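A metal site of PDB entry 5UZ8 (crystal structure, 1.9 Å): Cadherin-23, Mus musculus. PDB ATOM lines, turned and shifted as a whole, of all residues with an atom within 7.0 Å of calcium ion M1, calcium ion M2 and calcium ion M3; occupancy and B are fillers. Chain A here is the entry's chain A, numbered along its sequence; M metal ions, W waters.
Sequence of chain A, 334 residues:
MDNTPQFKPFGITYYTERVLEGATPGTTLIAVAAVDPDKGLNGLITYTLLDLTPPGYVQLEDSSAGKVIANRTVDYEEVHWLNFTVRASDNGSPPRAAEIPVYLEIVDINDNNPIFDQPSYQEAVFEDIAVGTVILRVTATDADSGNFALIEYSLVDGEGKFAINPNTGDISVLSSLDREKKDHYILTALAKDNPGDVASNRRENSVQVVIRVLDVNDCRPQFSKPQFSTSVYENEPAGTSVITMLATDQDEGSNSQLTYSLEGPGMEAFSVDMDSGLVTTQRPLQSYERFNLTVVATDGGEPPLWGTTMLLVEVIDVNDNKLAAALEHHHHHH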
ATOM      1  N   GLU A  21     -10.166 -28.612 -10.872  1.00  0.00           N
ATOM      2  CA  GLU A  21     -10.145 -29.086 -12.260  1.00  0.00           C
ATOM      3  C   GLU A  21     -10.070 -30.609 -12.297  1.00  0.00           C
ATOM      4  O   GLU A  21      -9.510 -31.240 -11.394  1.00  0.00           O
ATOM      5  CB  GLU A  21      -9.010 -28.455 -13.059  1.00  0.00           C
ATOM      6  CG  GLU A  21      -7.627 -28.896 -12.627  1.00  0.00           C
ATOM      7  CD  GLU A  21      -6.552 -28.518 -13.620  1.00  0.00           C
ATOM      8  OE1 GLU A  21      -5.414 -28.202 -13.171  1.00  0.00           O
ATOM      9  OE2 GLU A  21      -6.832 -28.574 -14.830  1.00  0.00           O
ATOM     10  N   GLY A  22     -10.707 -31.207 -13.290  1.00  0.00           N
ATOM     11  CA  GLY A  22     -10.744 -32.642 -13.440  1.00  0.00           C
ATOM     12  C   GLY A  22     -11.837 -33.363 -12.689  1.00  0.00           C
ATOM     13  O   GLY A  22     -11.926 -34.592 -12.787  1.00  0.00           O
ATOM     14  N   VAL A  74     -13.778 -30.055 -16.477  1.00  0.00           N
ATOM     15  CA  VAL A  74     -13.160 -28.745 -16.717  1.00  0.00           C
ATOM     16  C   VAL A  74     -11.644 -28.847 -16.548  1.00  0.00           C
ATOM     17  O   VAL A  74     -11.146 -29.636 -15.719  1.00  0.00           O
ATOM     18  CB  VAL A  74     -13.769 -27.677 -15.789  1.00  0.00           C
ATOM     19  CG1 VAL A  74     -13.305 -27.830 -14.352  1.00  0.00           C
ATOM     20  CG2 VAL A  74     -13.500 -26.279 -16.312  1.00  0.00           C
ATOM     21  N   ASP A  75     -10.949 -28.060 -17.340  1.00  0.00           N
ATOM     22  CA  ASP A  75      -9.501 -27.985 -17.382  1.00  0.00           C
ATOM     23  C   ASP A  75      -9.077 -26.555 -16.981  1.00  0.00           C
ATOM     24  O   ASP A  75      -9.387 -25.600 -17.688  1.00  0.00           O
ATOM     25  CB  ASP A  75      -9.048 -28.285 -18.811  1.00  0.00           C
ATOM     26  CG  ASP A  75      -7.521 -28.277 -18.981  1.00  0.00           C
ATOM     27  OD1 ASP A  75      -6.767 -28.099 -18.002  1.00  0.00           O
ATOM     28  OD2 ASP A  75      -7.079 -28.448 -20.122  1.00  0.00           O
ATOM     29  N   TYR A  76      -8.355 -26.410 -15.876  1.00  0.00           N
ATOM     30  CA  TYR A  76      -7.884 -25.113 -15.415  1.00  0.00           C
ATOM     31  C   TYR A  76      -7.034 -24.457 -16.486  1.00  0.00           C
ATOM     32  O   TYR A  76      -7.044 -23.249 -16.610  1.00  0.00           O
ATOM     33  CB  TYR A  76      -7.073 -25.235 -14.110  1.00  0.00           C
ATOM     34  CG  TYR A  76      -6.642 -23.900 -13.572  1.00  0.00           C
ATOM     35  CD1 TYR A  76      -7.528 -23.109 -12.788  1.00  0.00           C
ATOM     36  CD2 TYR A  76      -5.383 -23.374 -13.858  1.00  0.00           C
ATOM     37  CE1 TYR A  76      -7.129 -21.878 -12.309  1.00  0.00           C
ATOM     38  CE2 TYR A  76      -5.003 -22.159 -13.360  1.00  0.00           C
ATOM     39  CZ  TYR A  76      -5.872 -21.422 -12.612  1.00  0.00           C
ATOM     40  OH  TYR A  76      -5.466 -20.201 -12.145  1.00  0.00           O
ATOM     41  N   GLU A  77      -6.297 -25.247 -17.256  1.00  0.00           N
ATOM     42  CA  GLU A  77      -5.477 -24.684 -18.308  1.00  0.00           C
ATOM     43  C   GLU A  77      -6.302 -24.060 -19.459  1.00  0.00           C
ATOM     44  O   GLU A  77      -5.733 -23.349 -20.267  1.00  0.00           O
ATOM     45  CB  GLU A  77      -4.443 -25.693 -18.804  1.00  0.00           C
ATOM     46  CG  GLU A  77      -3.255 -25.879 -17.871  1.00  0.00           C
ATOM     47  CD  GLU A  77      -3.582 -26.473 -16.494  1.00  0.00           C
ATOM     48  OE1 GLU A  77      -3.280 -25.776 -15.528  1.00  0.00           O
ATOM     49  OE2 GLU A  77      -4.092 -27.618 -16.358  1.00  0.00           O
ATOM     50  N   GLU A  78      -7.637 -24.303 -19.480  1.00  0.00           N
ATOM     51  CA  GLU A  78      -8.554 -23.697 -20.472  1.00  0.00           C
ATOM     52  C   GLU A  78      -9.546 -22.726 -19.834  1.00  0.00           C
ATOM     53  O   GLU A  78      -9.911 -21.737 -20.462  1.00  0.00           O
ATOM     54  CB  GLU A  78      -9.356 -24.797 -21.186  1.00  0.00           C
ATOM     55  CG  GLU A  78      -8.502 -25.721 -22.029  1.00  0.00           C
ATOM     56  CD  GLU A  78      -7.750 -24.983 -23.123  1.00  0.00           C
ATOM     57  OE1 GLU A  78      -8.193 -23.880 -23.519  1.00  0.00           O
ATOM     58  OE2 GLU A  78      -6.710 -25.482 -23.585  1.00  0.00           O
ATOM     59  N   VAL A 107      -9.909 -24.558  -9.566  1.00  0.00           N
ATOM     60  CA  VAL A 107      -8.663 -24.660  -8.810  1.00  0.00           C
ATOM     61  C   VAL A 107      -7.693 -25.512  -9.607  1.00  0.00           C
ATOM     62  O   VAL A 107      -8.035 -26.616 -10.040  1.00  0.00           O
ATOM     63  CB  VAL A 107      -8.918 -25.320  -7.466  1.00  0.00           C
ATOM     64  CG1 VAL A 107      -7.620 -25.509  -6.678  1.00  0.00           C
ATOM     65  CG2 VAL A 107      -9.907 -24.489  -6.663  1.00  0.00           C
ATOM     66  N   ASP A 108      -6.496 -24.975  -9.815  1.00  0.00           N
ATOM     67  CA  ASP A 108      -5.431 -25.676 -10.536  1.00  0.00           C
ATOM     68  C   ASP A 108      -4.972 -26.881  -9.722  1.00  0.00           C
ATOM     69  O   ASP A 108      -4.742 -26.787  -8.501  1.00  0.00           O
ATOM     70  CB  ASP A 108      -4.267 -24.692 -10.707  1.00  0.00           C
ATOM     71  CG  ASP A 108      -3.080 -25.247 -11.484  1.00  0.00           C
ATOM     72  OD1 ASP A 108      -3.263 -26.025 -12.463  1.00  0.00           O
ATOM     73  OD2 ASP A 108      -1.944 -24.808 -11.158  1.00  0.00           O
ATOM     74  N   ILE A 109      -4.785 -28.005 -10.400  1.00  0.00           N
ATOM     75  CA  ILE A 109      -4.047 -29.153  -9.844  1.00  0.00           C
ATOM     76  C   ILE A 109      -2.782 -29.372 -10.663  1.00  0.00           C
ATOM     77  O   ILE A 109      -2.652 -28.881 -11.791  1.00  0.00           O
ATOM     78  CB  ILE A 109      -4.898 -30.459  -9.781  1.00  0.00           C
ATOM     79  CG1 ILE A 109      -5.052 -31.093 -11.161  1.00  0.00           C
ATOM     80  CG2 ILE A 109      -6.253 -30.202  -9.119  1.00  0.00           C
ATOM     81  CD1 ILE A 109      -5.916 -32.349 -11.207  1.00  0.00           C
ATOM     82  N   ASN A 110      -1.828 -30.101 -10.099  1.00  0.00           N
ATOM     83  CA  ASN A 110      -0.567 -30.308 -10.746  1.00  0.00           C
ATOM     84  C   ASN A 110      -0.643 -31.479 -11.711  1.00  0.00           C
ATOM     85  O   ASN A 110      -0.100 -32.566 -11.459  1.00  0.00           O
ATOM     86  CB  ASN A 110       0.560 -30.510  -9.719  1.00  0.00           C
ATOM     87  CG  ASN A 110       1.933 -30.484 -10.357  1.00  0.00           C
ATOM     88  OD1 ASN A 110       2.099 -29.899 -11.416  1.00  0.00           O
ATOM     89  ND2 ASN A 110       2.912 -31.099  -9.722  1.00  0.00           N
ATOM     90  N   ASP A 111      -1.307 -31.228 -12.846  1.00  0.00           N
ATOM     91  CA  ASP A 111      -1.549 -32.264 -13.863  1.00  0.00           C
ATOM     92  C   ASP A 111      -0.698 -32.122 -15.136  1.00  0.00           C
ATOM     93  O   ASP A 111      -0.912 -32.884 -16.091  1.00  0.00           O
ATOM     94  CB  ASP A 111      -3.052 -32.407 -14.169  1.00  0.00           C
ATOM     95  CG  ASP A 111      -3.717 -31.135 -14.709  1.00  0.00           C
ATOM     96  OD1 ASP A 111      -3.192 -30.003 -14.562  1.00  0.00           O
ATOM     97  OD2 ASP A 111      -4.859 -31.249 -15.213  1.00  0.00           O
ATOM     98  N   ASN A 112       0.255 -31.204 -15.149  1.00  0.00           N
ATOM     99  CA  ASN A 112       1.177 -31.094 -16.273  1.00  0.00           C
ATOM    100  C   ASN A 112       2.625 -31.271 -15.797  1.00  0.00           C
ATOM    101  O   ASN A 112       3.036 -30.673 -14.797  1.00  0.00           O
ATOM    102  CB  ASN A 112       1.032 -29.756 -16.992  1.00  0.00           C
ATOM    103  CG  ASN A 112      -0.293 -29.670 -17.751  1.00  0.00           C
ATOM    104  OD1 ASN A 112      -0.373 -30.103 -18.900  1.00  0.00           O
ATOM    105  ND2 ASN A 112      -1.347 -29.203 -17.067  1.00  0.00           N
ATOM    106  N   ASN A 113       3.387 -32.056 -16.539  1.00  0.00           N
ATOM    107  CA  ASN A 113       4.806 -32.245 -16.266  1.00  0.00           C
ATOM    108  C   ASN A 113       5.582 -31.109 -16.898  1.00  0.00           C
ATOM    109  O   ASN A 113       5.180 -30.638 -17.969  1.00  0.00           O
ATOM    110  CB  ASN A 113       5.325 -33.530 -16.905  1.00  0.00           C
ATOM    111  CG  ASN A 113       4.787 -34.781 -16.233  1.00  0.00           C
ATOM    112  OD1 ASN A 113       3.609 -34.908 -16.059  1.00  0.00           O
ATOM    113  ND2 ASN A 113       5.671 -35.693 -15.853  1.00  0.00           N
ATOM    114  N   PRO A 114       6.767 -30.783 -16.335  1.00  0.00           N
ATOM    115  CA  PRO A 114       7.690 -29.961 -17.129  1.00  0.00           C
ATOM    116  C   PRO A 114       8.139 -30.731 -18.345  1.00  0.00           C
ATOM    117  O   PRO A 114       8.370 -31.954 -18.261  1.00  0.00           O
ATOM    118  CB  PRO A 114       8.867 -29.696 -16.182  1.00  0.00           C
ATOM    119  CG  PRO A 114       8.449 -30.142 -14.846  1.00  0.00           C
ATOM    120  CD  PRO A 114       7.331 -31.173 -15.043  1.00  0.00           C
ATOM    121  N   ASP A 142       6.229 -25.569 -18.135  1.00  0.00           N
ATOM    122  CA  ASP A 142       5.190 -26.268 -17.368  1.00  0.00           C
ATOM    123  C   ASP A 142       3.874 -25.469 -17.489  1.00  0.00           C
ATOM    124  O   ASP A 142       3.808 -24.291 -17.135  1.00  0.00           O
ATOM    125  CB  ASP A 142       5.622 -26.411 -15.933  1.00  0.00           C
ATOM    126  CG  ASP A 142       4.731 -27.365 -15.124  1.00  0.00           C
ATOM    127  OD1 ASP A 142       3.510 -27.098 -15.001  1.00  0.00           O
ATOM    128  OD2 ASP A 142       5.248 -28.318 -14.506  1.00  0.00           O
ATOM    129  N   ALA A 143       2.839 -26.145 -17.962  1.00  0.00           N
ATOM    130  CA  ALA A 143       1.543 -25.524 -18.238  1.00  0.00           C
ATOM    131  C   ALA A 143       0.628 -25.225 -17.045  1.00  0.00           C
ATOM    132  O   ALA A 143      -0.379 -24.561 -17.216  1.00  0.00           O
ATOM    133  CB  ALA A 143       0.795 -26.392 -19.267  1.00  0.00           C
ATOM    134  N   ASP A 144       0.994 -25.652 -15.832  1.00  0.00           N
ATOM    135  CA  ASP A 144       0.226 -25.320 -14.640  1.00  0.00           C
ATOM    136  C   ASP A 144       0.487 -23.869 -14.201  1.00  0.00           C
ATOM    137  O   ASP A 144       1.055 -23.070 -14.974  1.00  0.00           O
ATOM    138  CB  ASP A 144       0.535 -26.334 -13.520  1.00  0.00           C
ATOM    139  CG  ASP A 144       0.155 -27.742 -13.913  1.00  0.00           C
ATOM    140  OD1 ASP A 144      -0.981 -27.948 -14.377  1.00  0.00           O
ATOM    141  OD2 ASP A 144       1.018 -28.643 -13.808  1.00  0.00           O
ATOM    142  N   SER A 145       0.059 -23.539 -13.001  1.00  0.00           N
ATOM    143  CA  SER A 145       0.181 -22.219 -12.437  1.00  0.00           C
ATOM    144  C   SER A 145       0.836 -22.265 -11.044  1.00  0.00           C
ATOM    145  O   SER A 145       0.869 -23.292 -10.375  1.00  0.00           O
ATOM    146  CB  SER A 145      -1.181 -21.553 -12.382  1.00  0.00           C
ATOM    147  OG  SER A 145      -1.660 -21.365 -13.741  1.00  0.00           O
ATOM    148  N   ASN A 147       3.080 -22.574  -7.880  1.00  0.00           N
ATOM    149  CA  ASN A 147       4.158 -23.525  -7.504  1.00  0.00           C
ATOM    150  C   ASN A 147       4.187 -24.769  -8.390  1.00  0.00           C
ATOM    151  O   ASN A 147       5.260 -25.300  -8.652  1.00  0.00           O
ATOM    152  CB  ASN A 147       4.068 -23.969  -6.044  1.00  0.00           C
ATOM    153  CG  ASN A 147       5.429 -24.199  -5.443  1.00  0.00           C
ATOM    154  OD1 ASN A 147       6.177 -23.229  -5.295  1.00  0.00           O
ATOM    155  ND2 ASN A 147       5.783 -25.445  -5.117  1.00  0.00           N
ATOM    156  N   PHE A 148       3.025 -25.187  -8.869  1.00  0.00           N
ATOM    157  CA  PHE A 148       2.921 -26.320  -9.749  1.00  0.00           C
ATOM    158  C   PHE A 148       3.601 -26.150 -11.096  1.00  0.00           C
ATOM    159  O   PHE A 148       3.794 -27.139 -11.826  1.00  0.00           O
ATOM    160  CB  PHE A 148       1.435 -26.652  -9.951  1.00  0.00           C
ATOM    161  CG  PHE A 148       0.708 -27.085  -8.722  1.00  0.00           C
ATOM    162  CD1 PHE A 148       1.368 -27.650  -7.617  1.00  0.00           C
ATOM    163  CD2 PHE A 148      -0.670 -27.034  -8.701  1.00  0.00           C
ATOM    164  CE1 PHE A 148       0.660 -28.096  -6.517  1.00  0.00           C
ATOM    165  CE2 PHE A 148      -1.387 -27.495  -7.611  1.00  0.00           C
ATOM    166  CZ  PHE A 148      -0.724 -28.023  -6.501  1.00  0.00           C
ATOM    167  N   ALA A 149       3.961 -24.912 -11.448  1.00  0.00           N
ATOM    168  CA  ALA A 149       4.674 -24.635 -12.722  1.00  0.00           C
ATOM    169  C   ALA A 149       6.102 -24.085 -12.515  1.00  0.00           C
ATOM    170  O   ALA A 149       6.763 -23.710 -13.500  1.00  0.00           O
ATOM    171  CB  ALA A 149       3.850 -23.654 -13.562  1.00  0.00           C
ATOM    172  N   LEU A 150       6.561 -24.040 -11.257  1.00  0.00           N
ATOM    173  CA  LEU A 150       7.928 -23.682 -10.967  1.00  0.00           C
ATOM    174  C   LEU A 150       8.781 -24.919 -11.157  1.00  0.00           C
ATOM    175  O   LEU A 150       8.388 -25.998 -10.724  1.00  0.00           O
ATOM    176  CB  LEU A 150       8.104 -23.157  -9.557  1.00  0.00           C
ATOM    177  CG  LEU A 150       7.374 -21.855  -9.260  1.00  0.00           C
ATOM    178  CD1 LEU A 150       7.709 -21.376  -7.852  1.00  0.00           C
ATOM    179  CD2 LEU A 150       7.797 -20.794 -10.290  1.00  0.00           C
ATOM    180  N   ASP A 193       8.911 -30.180 -11.121  1.00  0.00           N
ATOM    181  CA  ASP A 193       8.067 -29.057 -10.752  1.00  0.00           C
ATOM    182  C   ASP A 193       7.761 -29.056  -9.262  1.00  0.00           C
ATOM    183  O   ASP A 193       8.251 -29.912  -8.524  1.00  0.00           O
ATOM    184  CB  ASP A 193       6.813 -29.007 -11.655  1.00  0.00           C
ATOM    185  CG  ASP A 193       5.822 -30.109 -11.348  1.00  0.00           C
ATOM    186  OD1 ASP A 193       5.912 -30.767 -10.283  1.00  0.00           O
ATOM    187  OD2 ASP A 193       4.915 -30.276 -12.190  1.00  0.00           O
ATOM    188  N   ASN A 194       6.949 -28.097  -8.818  1.00  0.00           N
ATOM    189  CA  ASN A 194       6.338 -28.064  -7.499  1.00  0.00           C
ATOM    190  C   ASN A 194       7.348 -28.163  -6.340  1.00  0.00           C
ATOM    191  O   ASN A 194       7.265 -29.055  -5.489  1.00  0.00           O
ATOM    192  CB  ASN A 194       5.219 -29.155  -7.393  1.00  0.00           C
ATOM    193  CG  ASN A 194       4.317 -28.978  -6.180  1.00  0.00           C
ATOM    194  OD1 ASN A 194       4.217 -27.913  -5.575  1.00  0.00           O
ATOM    195  ND2 ASN A 194       3.617 -30.083  -5.821  1.00  0.00           N
ATOM    196  N   ASN A 201       3.671 -35.410  -5.186  1.00  0.00           N
ATOM    197  CA  ASN A 201       2.921 -34.354  -5.907  1.00  0.00           C
ATOM    198  C   ASN A 201       3.878 -33.546  -6.785  1.00  0.00           C
ATOM    199  O   ASN A 201       3.509 -32.503  -7.260  1.00  0.00           O
ATOM    200  CB  ASN A 201       2.070 -33.435  -4.931  1.00  0.00           C
ATOM    201  CG  ASN A 201       0.898 -32.626  -5.634  1.00  0.00           C
ATOM    202  OD1 ASN A 201       0.311 -33.013  -6.650  1.00  0.00           O
ATOM    203  ND2 ASN A 201       0.557 -31.502  -5.030  1.00  0.00           N
ATOM    204  N   ARG A 203       6.054 -33.595 -10.397  1.00  0.00           N
ATOM    205  CA  ARG A 203       6.175 -34.212 -11.700  1.00  0.00           C
ATOM    206  C   ARG A 203       7.501 -33.811 -12.325  1.00  0.00           C
ATOM    207  O   ARG A 203       8.068 -32.763 -12.030  1.00  0.00           O
ATOM    208  CB  ARG A 203       5.024 -33.754 -12.614  1.00  0.00           C
ATOM    209  CG  ARG A 203       3.685 -34.329 -12.271  1.00  0.00           C
ATOM    210  CD  ARG A 203       2.566 -33.733 -13.113  1.00  0.00           C
ATOM    211  NE  ARG A 203       1.296 -34.440 -12.917  1.00  0.00           N
ATOM    212  CZ  ARG A 203       0.923 -35.564 -13.521  1.00  0.00           C
ATOM    213  NH1 ARG A 203      -0.264 -36.076 -13.262  1.00  0.00           N
ATOM    214  NH2 ARG A 203       1.691 -36.164 -14.418  1.00  0.00           N
HETATM  215 CA    CA M   1      -5.439 -29.445 -16.598  1.00  0.00          CA
HETATM  216 CA    CA M   2      -3.237 -27.733 -13.910  1.00  0.00          CA
HETATM  217 CA    CA M   3       3.309 -28.993 -13.254  1.00  0.00          CA
HETATM  218  O   HOH W   1      -3.918 -30.106 -18.285  1.00  0.00           O
HETATM  219  O   HOH W   2      -6.951 -31.071 -17.628  1.00  0.00           O
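The side-chain carboxylate (OD2) of Asp 108 lies within hydrogen-bond range of the backbone NH (N) of Ser 145, at 3.0 Å. The side-chain carboxylate (OE2) of Glu 77 sits close to the side-chain amide nitrogen (ND2) of Asn 112, 3.2 Å away. The side-chain amide nitrogen (ND2) of Asn 112 sits close to the side-chain carboxylate (OD1) of Asp 111. OD1 of Asp 193 is in hydrogen-bond range of N of Arg 203, at 2.8 Å. N of Tyr 76 lies close to OE2 of Glu 21 (2.8 Å). O of Val 107 lies within hydrogen-bond range of N of Glu 21 (3.0 Å). The guanidinium group of Arg 203 sits at hydrogen-bond distance from the backbone carbonyl oxygen of Asn 110 (2.8 Å). ND2 of Asn 110 lies within hydrogen-bond range of O of Asn 201, 2.9 Å away.
The nearest printed residue that does not touch calcium ion M1 is Asn 112 (4.1 Å).
Along chain A the residues within 4 Å of calcium ion M3 span positions 110 to 193.
Calcium ion M1 is bound by the side-chain carboxylate (OE2) of Glu 77 (2.3 Å), the side-chain carboxylate (OD2) of Asp 111 (2.3 Å), the side-chain carboxylate (OD1) of Asp 75 (2.4 Å), water W1 (2.4 Å), the side-chain carboxylate (OE2) of Glu 21 (2.4 Å) and water W2 (2.4 Å). Calcium ion M1 has six donor atoms within binding distance. Slightly farther from calcium ion M1 lies OD1 of Asp 111 (3.1 Å).
Calcium ion M2 is bound by OD1 of Asp 108 (2.2 Å), OD1 of Asp 144 (2.3 Å), OE1 of Glu 21 (2.3 Å), OD1 of Asp 111 (2.4 Å), O of Ile 109 (2.5 Å), OE1 of Glu 77 (2.5 Å) and OE2 of Glu 77 (2.6 Å). Calcium ion M2 has seven donor atoms within binding distance.
Calcium ion M3 is bound by the backbone carbonyl oxygen (O) of Asn 112 (2.3 Å), the side-chain carboxylate (OD2) of Asp 193 (2.3 Å), the side-chain amide oxygen (OD1) of Asn 110 (2.4 Å), the side-chain carboxylate (OD2) of Asp 144 (2.4 Å), the backbone carbonyl oxygen (O) of Phe 148 (2.4 Å), the side-chain carboxylate (OD2) of Asp 142 (2.4 Å) and the side-chain carboxylate (OD1) of Asp 142 (2.6 Å). Calcium ion M3 has seven donor atoms within binding distance.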
